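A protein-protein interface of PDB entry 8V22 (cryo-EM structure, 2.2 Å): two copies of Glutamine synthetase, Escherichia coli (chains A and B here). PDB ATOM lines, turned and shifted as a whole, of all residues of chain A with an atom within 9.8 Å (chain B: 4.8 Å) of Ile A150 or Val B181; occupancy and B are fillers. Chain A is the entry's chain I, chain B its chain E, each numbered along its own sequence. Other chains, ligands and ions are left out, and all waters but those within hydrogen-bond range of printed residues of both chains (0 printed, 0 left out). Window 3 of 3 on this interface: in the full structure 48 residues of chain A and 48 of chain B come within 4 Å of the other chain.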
ATOM      1  N   GLY A 147      29.251  37.431 -15.945  1.00  0.00           N
ATOM      2  CA  GLY A 147      27.895  37.211 -16.400  1.00  0.00           C
ATOM      3  C   GLY A 147      27.590  35.736 -16.491  1.00  0.00           C
ATOM      4  O   GLY A 147      28.491  34.893 -16.487  1.00  0.00           O
ATOM      5  N   SER A 148      26.297  35.438 -16.566  1.00  0.00           N
ATOM      6  CA  SER A 148      25.824  34.075 -16.738  1.00  0.00           C
ATOM      7  C   SER A 148      24.513  34.112 -17.501  1.00  0.00           C
ATOM      8  O   SER A 148      23.741  35.067 -17.390  1.00  0.00           O
ATOM      9  CB  SER A 148      25.634  33.368 -15.394  1.00  0.00           C
ATOM     10  OG  SER A 148      24.587  33.965 -14.652  1.00  0.00           O
ATOM     11  N   SER A 149      24.269  33.065 -18.278  1.00  0.00           N
ATOM     12  CA  SER A 149      23.026  32.930 -19.022  1.00  0.00           C
ATOM     13  C   SER A 149      22.853  31.460 -19.379  1.00  0.00           C
ATOM     14  O   SER A 149      23.613  30.600 -18.922  1.00  0.00           O
ATOM     15  CB  SER A 149      23.031  33.835 -20.258  1.00  0.00           C
ATOM     16  OG  SER A 149      24.069  33.481 -21.152  1.00  0.00           O
ATOM     17  N   ILE A 150      21.843  31.167 -20.198  1.00  0.00           N
ATOM     18  CA  ILE A 150      21.635  29.794 -20.638  1.00  0.00           C
ATOM     19  C   ILE A 150      22.790  29.332 -21.513  1.00  0.00           C
ATOM     20  O   ILE A 150      23.147  28.148 -21.508  1.00  0.00           O
ATOM     21  CB  ILE A 150      20.289  29.666 -21.374  1.00  0.00           C
ATOM     22  CG1 ILE A 150      19.986  28.195 -21.658  1.00  0.00           C
ATOM     23  CG2 ILE A 150      20.305  30.469 -22.666  1.00  0.00           C
ATOM     24  CD1 ILE A 150      18.551  27.927 -22.026  1.00  0.00           C
ATOM     25  N   SER A 151      23.390  30.244 -22.274  1.00  0.00           N
ATOM     26  CA  SER A 151      24.426  29.885 -23.232  1.00  0.00           C
ATOM     27  C   SER A 151      25.793  29.688 -22.594  1.00  0.00           C
ATOM     28  O   SER A 151      26.689  29.150 -23.254  1.00  0.00           O
ATOM     29  CB  SER A 151      24.530  30.966 -24.307  1.00  0.00           C
ATOM     30  OG  SER A 151      24.816  32.224 -23.724  1.00  0.00           O
ATOM     31  N   GLY A 152      25.981  30.096 -21.349  1.00  0.00           N
ATOM     32  CA  GLY A 152      27.275  29.969 -20.714  1.00  0.00           C
ATOM     33  C   GLY A 152      27.426  30.977 -19.591  1.00  0.00           C
ATOM     34  O   GLY A 152      26.458  31.582 -19.134  1.00  0.00           O
ATOM     35  N   SER A 153      28.674  31.133 -19.155  1.00  0.00           N
ATOM     36  CA  SER A 153      28.991  32.029 -18.052  1.00  0.00           C
ATOM     37  C   SER A 153      30.468  32.386 -18.098  1.00  0.00           C
ATOM     38  O   SER A 153      31.300  31.572 -18.495  1.00  0.00           O
ATOM     39  CB  SER A 153      28.652  31.391 -16.704  1.00  0.00           C
ATOM     40  OG  SER A 153      29.370  30.182 -16.533  1.00  0.00           O
ATOM     41  N   HIS A 154      30.793  33.594 -17.648  1.00  0.00           N
ATOM     42  CA  HIS A 154      32.171  34.058 -17.703  1.00  0.00           C
ATOM     43  C   HIS A 154      32.476  35.014 -16.561  1.00  0.00           C
ATOM     44  O   HIS A 154      31.590  35.688 -16.032  1.00  0.00           O
ATOM     45  CB  HIS A 154      32.471  34.746 -19.037  1.00  0.00           C
ATOM     46  CG  HIS A 154      31.799  36.072 -19.197  1.00  0.00           C
ATOM     47  ND1 HIS A 154      32.483  37.267 -19.133  1.00  0.00           N
ATOM     48  CD2 HIS A 154      30.507  36.392 -19.441  1.00  0.00           C
ATOM     49  CE1 HIS A 154      31.639  38.266 -19.316  1.00  0.00           C
ATOM     50  NE2 HIS A 154      30.433  37.762 -19.507  1.00  0.00           N
ATOM     51  N   ARG A 458      22.109  28.501  -6.062  1.00  0.00           N
ATOM     52  CA  ARG A 458      22.498  29.079  -7.347  1.00  0.00           C
ATOM     53  C   ARG A 458      23.864  28.558  -7.780  1.00  0.00           C
ATOM     54  O   ARG A 458      24.032  28.060  -8.906  1.00  0.00           O
ATOM     55  CB  ARG A 458      22.508  30.608  -7.259  1.00  0.00           C
ATOM     56  CG  ARG A 458      21.122  31.231  -7.286  1.00  0.00           C
ATOM     57  CD  ARG A 458      21.122  32.653  -7.833  1.00  0.00           C
ATOM     58  NE  ARG A 458      21.495  32.713  -9.243  1.00  0.00           N
ATOM     59  CZ  ARG A 458      22.562  33.337  -9.727  1.00  0.00           C
ATOM     60  NH1 ARG A 458      23.399  33.998  -8.943  1.00  0.00           N
ATOM     61  NH2 ARG A 458      22.793  33.303 -11.036  1.00  0.00           N
ATOM     62  N   THR A 462      24.589  26.036 -11.067  1.00  0.00           N
ATOM     63  CA  THR A 462      25.114  26.579 -12.322  1.00  0.00           C
ATOM     64  C   THR A 462      26.358  25.809 -12.769  1.00  0.00           C
ATOM     65  O   THR A 462      27.289  25.639 -11.975  1.00  0.00           O
ATOM     66  CB  THR A 462      25.451  28.055 -12.190  1.00  0.00           C
ATOM     67  OG1 THR A 462      24.416  28.724 -11.461  1.00  0.00           O
ATOM     68  CG2 THR A 462      25.590  28.680 -13.564  1.00  0.00           C
ATOM     69  N   PRO A 463      26.416  25.340 -14.020  1.00  0.00           N
ATOM     70  CA  PRO A 463      27.596  24.598 -14.483  1.00  0.00           C
ATOM     71  C   PRO A 463      28.864  25.437 -14.445  1.00  0.00           C
ATOM     72  O   PRO A 463      28.824  26.669 -14.423  1.00  0.00           O
ATOM     73  CB  PRO A 463      27.235  24.217 -15.920  1.00  0.00           C
ATOM     74  CG  PRO A 463      25.775  24.211 -15.955  1.00  0.00           C
ATOM     75  CD  PRO A 463      25.328  25.280 -15.011  1.00  0.00           C
ATOM     76  N   PHE A 468      33.328  22.025 -17.892  1.00  0.00           N
ATOM     77  CA  PHE A 468      33.449  21.787 -19.329  1.00  0.00           C
ATOM     78  C   PHE A 468      34.849  21.315 -19.693  1.00  0.00           C
ATOM     79  O   PHE A 468      35.004  20.320 -20.412  1.00  0.00           O
ATOM     80  CB  PHE A 468      33.087  23.039 -20.123  1.00  0.00           C
ATOM     81  CG  PHE A 468      31.628  23.376 -20.090  1.00  0.00           C
ATOM     82  CD1 PHE A 468      31.049  23.926 -18.966  1.00  0.00           C
ATOM     83  CD2 PHE A 468      30.837  23.154 -21.201  1.00  0.00           C
ATOM     84  CE1 PHE A 468      29.712  24.234 -18.947  1.00  0.00           C
ATOM     85  CE2 PHE A 468      29.502  23.462 -21.186  1.00  0.00           C
ATOM     86  CZ  PHE A 468      28.940  24.003 -20.059  1.00  0.00           C
ATOM     87  N   ALA B 163      17.658  28.986 -28.500  1.00  0.00           N
ATOM     88  CA  ALA B 163      16.639  30.030 -28.496  1.00  0.00           C
ATOM     89  C   ALA B 163      17.262  31.416 -28.403  1.00  0.00           C
ATOM     90  O   ALA B 163      16.728  32.377 -28.970  1.00  0.00           O
ATOM     91  CB  ALA B 163      15.667  29.804 -27.339  1.00  0.00           C
ATOM     92  N   TRP B 164      18.403  31.535 -27.725  1.00  0.00           N
ATOM     93  CA  TRP B 164      19.053  32.827 -27.583  1.00  0.00           C
ATOM     94  C   TRP B 164      19.532  33.384 -28.913  1.00  0.00           C
ATOM     95  O   TRP B 164      19.864  34.572 -28.983  1.00  0.00           O
ATOM     96  CB  TRP B 164      20.239  32.721 -26.624  1.00  0.00           C
ATOM     97  CG  TRP B 164      21.285  31.734 -27.044  1.00  0.00           C
ATOM     98  CD1 TRP B 164      22.353  31.971 -27.859  1.00  0.00           C
ATOM     99  CD2 TRP B 164      21.370  30.359 -26.664  1.00  0.00           C
ATOM    100  NE1 TRP B 164      23.095  30.828 -28.010  1.00  0.00           N
ATOM    101  CE2 TRP B 164      22.512  29.822 -27.286  1.00  0.00           C
ATOM    102  CE3 TRP B 164      20.590  29.527 -25.860  1.00  0.00           C
ATOM    103  CZ2 TRP B 164      22.891  28.495 -27.128  1.00  0.00           C
ATOM    104  CZ3 TRP B 164      20.968  28.212 -25.705  1.00  0.00           C
ATOM    105  CH2 TRP B 164      22.109  27.709 -26.334  1.00  0.00           C
ATOM    106  N   PRO B 179      13.737  25.713 -31.554  1.00  0.00           N
ATOM    107  CA  PRO B 179      13.060  25.226 -30.349  1.00  0.00           C
ATOM    108  C   PRO B 179      13.112  26.264 -29.241  1.00  0.00           C
ATOM    109  O   PRO B 179      14.107  26.972 -29.075  1.00  0.00           O
ATOM    110  CB  PRO B 179      13.847  23.966 -29.977  1.00  0.00           C
ATOM    111  CG  PRO B 179      14.621  23.602 -31.180  1.00  0.00           C
ATOM    112  CD  PRO B 179      14.877  24.862 -31.926  1.00  0.00           C
ATOM    113  N   ALA B 180      12.027  26.352 -28.482  1.00  0.00           N
ATOM    114  CA  ALA B 180      12.031  27.164 -27.281  1.00  0.00           C
ATOM    115  C   ALA B 180      12.709  26.402 -26.147  1.00  0.00           C
ATOM    116  O   ALA B 180      12.966  25.199 -26.237  1.00  0.00           O
ATOM    117  CB  ALA B 180      10.607  27.554 -26.891  1.00  0.00           C
ATOM    118  N   VAL B 181      13.007  27.117 -25.062  1.00  0.00           N
ATOM    119  CA  VAL B 181      13.605  26.468 -23.906  1.00  0.00           C
ATOM    120  C   VAL B 181      12.635  25.424 -23.378  1.00  0.00           C
ATOM    121  O   VAL B 181      11.473  25.726 -23.075  1.00  0.00           O
ATOM    122  CB  VAL B 181      13.968  27.506 -22.834  1.00  0.00           C
ATOM    123  CG1 VAL B 181      14.512  26.822 -21.588  1.00  0.00           C
ATOM    124  CG2 VAL B 181      14.977  28.499 -23.380  1.00  0.00           C
ATOM    125  N   LYS B 182      13.106  24.183 -23.274  1.00  0.00           N
ATOM    126  CA  LYS B 182      12.269  23.058 -22.858  1.00  0.00           C
ATOM    127  C   LYS B 182      11.109  22.846 -23.827  1.00  0.00           C
ATOM    128  O   LYS B 182      10.000  22.491 -23.426  1.00  0.00           O
ATOM    129  CB  LYS B 182      11.751  23.254 -21.434  1.00  0.00           C
ATOM    130  CG  LYS B 182      12.837  23.285 -20.377  1.00  0.00           C
ATOM    131  CD  LYS B 182      12.254  23.381 -18.977  1.00  0.00           C
ATOM    132  CE  LYS B 182      11.578  22.086 -18.557  1.00  0.00           C
ATOM    133  NZ  LYS B 182      11.191  22.102 -17.119  1.00  0.00           N
ATOM    134  N   GLY B 183      11.366  23.060 -25.115  1.00  0.00           N
ATOM    135  CA  GLY B 183      10.336  22.912 -26.122  1.00  0.00           C
ATOM    136  C   GLY B 183      10.820  22.231 -27.384  1.00  0.00           C
ATOM    137  O   GLY B 183      10.292  22.479 -28.472  1.00  0.00           O
ATOM    138  N   THR B 221      16.831  22.870 -25.791  1.00  0.00           N
ATOM    139  CA  THR B 221      16.736  23.710 -26.979  1.00  0.00           C
ATOM    140  C   THR B 221      17.968  23.622 -27.871  1.00  0.00           C
ATOM    141  O   THR B 221      17.836  23.585 -29.099  1.00  0.00           O
ATOM    142  CB  THR B 221      16.504  25.171 -26.573  1.00  0.00           C
ATOM    143  OG1 THR B 221      16.218  25.954 -27.736  1.00  0.00           O
ATOM    144  CG2 THR B 221      17.728  25.747 -25.876  1.00  0.00           C
ATOM    145  N   MET B 266      24.008  23.145 -19.915  1.00  0.00           N
ATOM    146  CA  MET B 266      23.343  24.433 -19.782  1.00  0.00           C
ATOM    147  C   MET B 266      22.480  24.455 -18.533  1.00  0.00           C
ATOM    148  O   MET B 266      21.889  23.440 -18.155  1.00  0.00           O
ATOM    149  CB  MET B 266      22.473  24.735 -21.001  1.00  0.00           C
ATOM    150  CG  MET B 266      23.222  24.747 -22.315  1.00  0.00           C
ATOM    151  SD  MET B 266      22.155  25.164 -23.701  1.00  0.00           S
ATOM    152  CE  MET B 266      21.118  23.712 -23.774  1.00  0.00           C
ATOM    153  N   PHE B 267      22.416  25.619 -17.897  1.00  0.00           N
ATOM    154  CA  PHE B 267      21.517  25.840 -16.777  1.00  0.00           C
ATOM    155  C   PHE B 267      20.193  26.388 -17.285  1.00  0.00           C
ATOM    156  O   PHE B 267      20.153  27.161 -18.245  1.00  0.00           O
ATOM    157  CB  PHE B 267      22.127  26.809 -15.768  1.00  0.00           C
ATOM    158  CG  PHE B 267      21.221  27.121 -14.619  1.00  0.00           C
ATOM    159  CD1 PHE B 267      20.972  26.175 -13.645  1.00  0.00           C
ATOM    160  CD2 PHE B 267      20.608  28.354 -14.518  1.00  0.00           C
ATOM    161  CE1 PHE B 267      20.136  26.456 -12.590  1.00  0.00           C
ATOM    162  CE2 PHE B 267      19.771  28.639 -13.464  1.00  0.00           C
ATOM    163  CZ  PHE B 267      19.534  27.687 -12.499  1.00  0.00           C
ATOM    164  N   GLY B 268      19.108  25.981 -16.636  1.00  0.00           N
ATOM    165  CA  GLY B 268      17.785  26.380 -17.053  1.00  0.00           C
ATOM    166  C   GLY B 268      17.193  25.540 -18.159  1.00  0.00           C
ATOM    167  O   GLY B 268      16.054  25.797 -18.567  1.00  0.00           O
ATOM    168  N   ASP B 269      17.926  24.552 -18.662  1.00  0.00           N
ATOM    169  CA  ASP B 269      17.428  23.642 -19.675  1.00  0.00           C
ATOM    170  C   ASP B 269      17.700  22.213 -19.229  1.00  0.00           C
ATOM    171  O   ASP B 269      18.591  21.953 -18.416  1.00  0.00           O
ATOM    172  CB  ASP B 269      18.074  23.905 -21.040  1.00  0.00           C
ATOM    173  CG  ASP B 269      17.166  23.539 -22.195  1.00  0.00           C
ATOM    174  OD1 ASP B 269      16.026  23.098 -21.946  1.00  0.00           O
ATOM    175  OD2 ASP B 269      17.593  23.698 -23.358  1.00  0.00           O
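The side-chain hydroxyl (OG) of Ser A149 lies within hydrogen-bond range of the side-chain hydroxyl (OG) of Ser A151 (3.0 Å).
Among the printed residues, pairs that only touch across the chains: Ile A150 with Trp B164, Ile A150 with Met B266, Ile A150 with Phe B267, Pro A463 with Phe B267, Ser A151 with Trp B164 and Ile A150 with Val B181.
Of chain A, only Ile A150 comes within 4 Å of Val B181. No residue of chain A comes within 4 Å of Gly B268. Printed residues of chain B within 4 Å of Pro A463: Phe B267 (3.6 Å). Of the printed residues of chain A, Met B266 touches Ile A150 (3.5 Å). Of the printed residues of chain A, Trp B164 touches Ile A150 and Ser A151. Of the printed residues of chain B, Ser A151 touches Trp B164. Pro B179 touches none of the printed residues of chain A. The nearest printed residue of chain B that does not touch Ser A151 is Met B266 (5.3 Å).
Of the 12 printed residues of chain B, 4 touch a printed residue of chain A. Hydrophobic or aromatic side chains of chain B that line the printed part of chain A: Trp B164, Val B181, Met B266 and Phe B267. Of the 12 printed residues of chain A, 3 touch a printed residue of chain B. Printed residues of chain A that touch a printed residue of chain B: Ile A150, Ser A151 and Pro A463. Hydrophobic or aromatic side chains of chain A that line the printed part of chain B: Ile A150 and Pro A463. Among the printed residues, 6 pairs touch across the chains. Among the printed residues, no Asp or Glu carboxylate lies within 4 Å of a Lys or Arg side-chain nitrogen of the other chain.
No position is printed for both chains. Of the 6 pairs that touch across the chains among the printed residues, none has its exchanged pair printed and touching as well.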
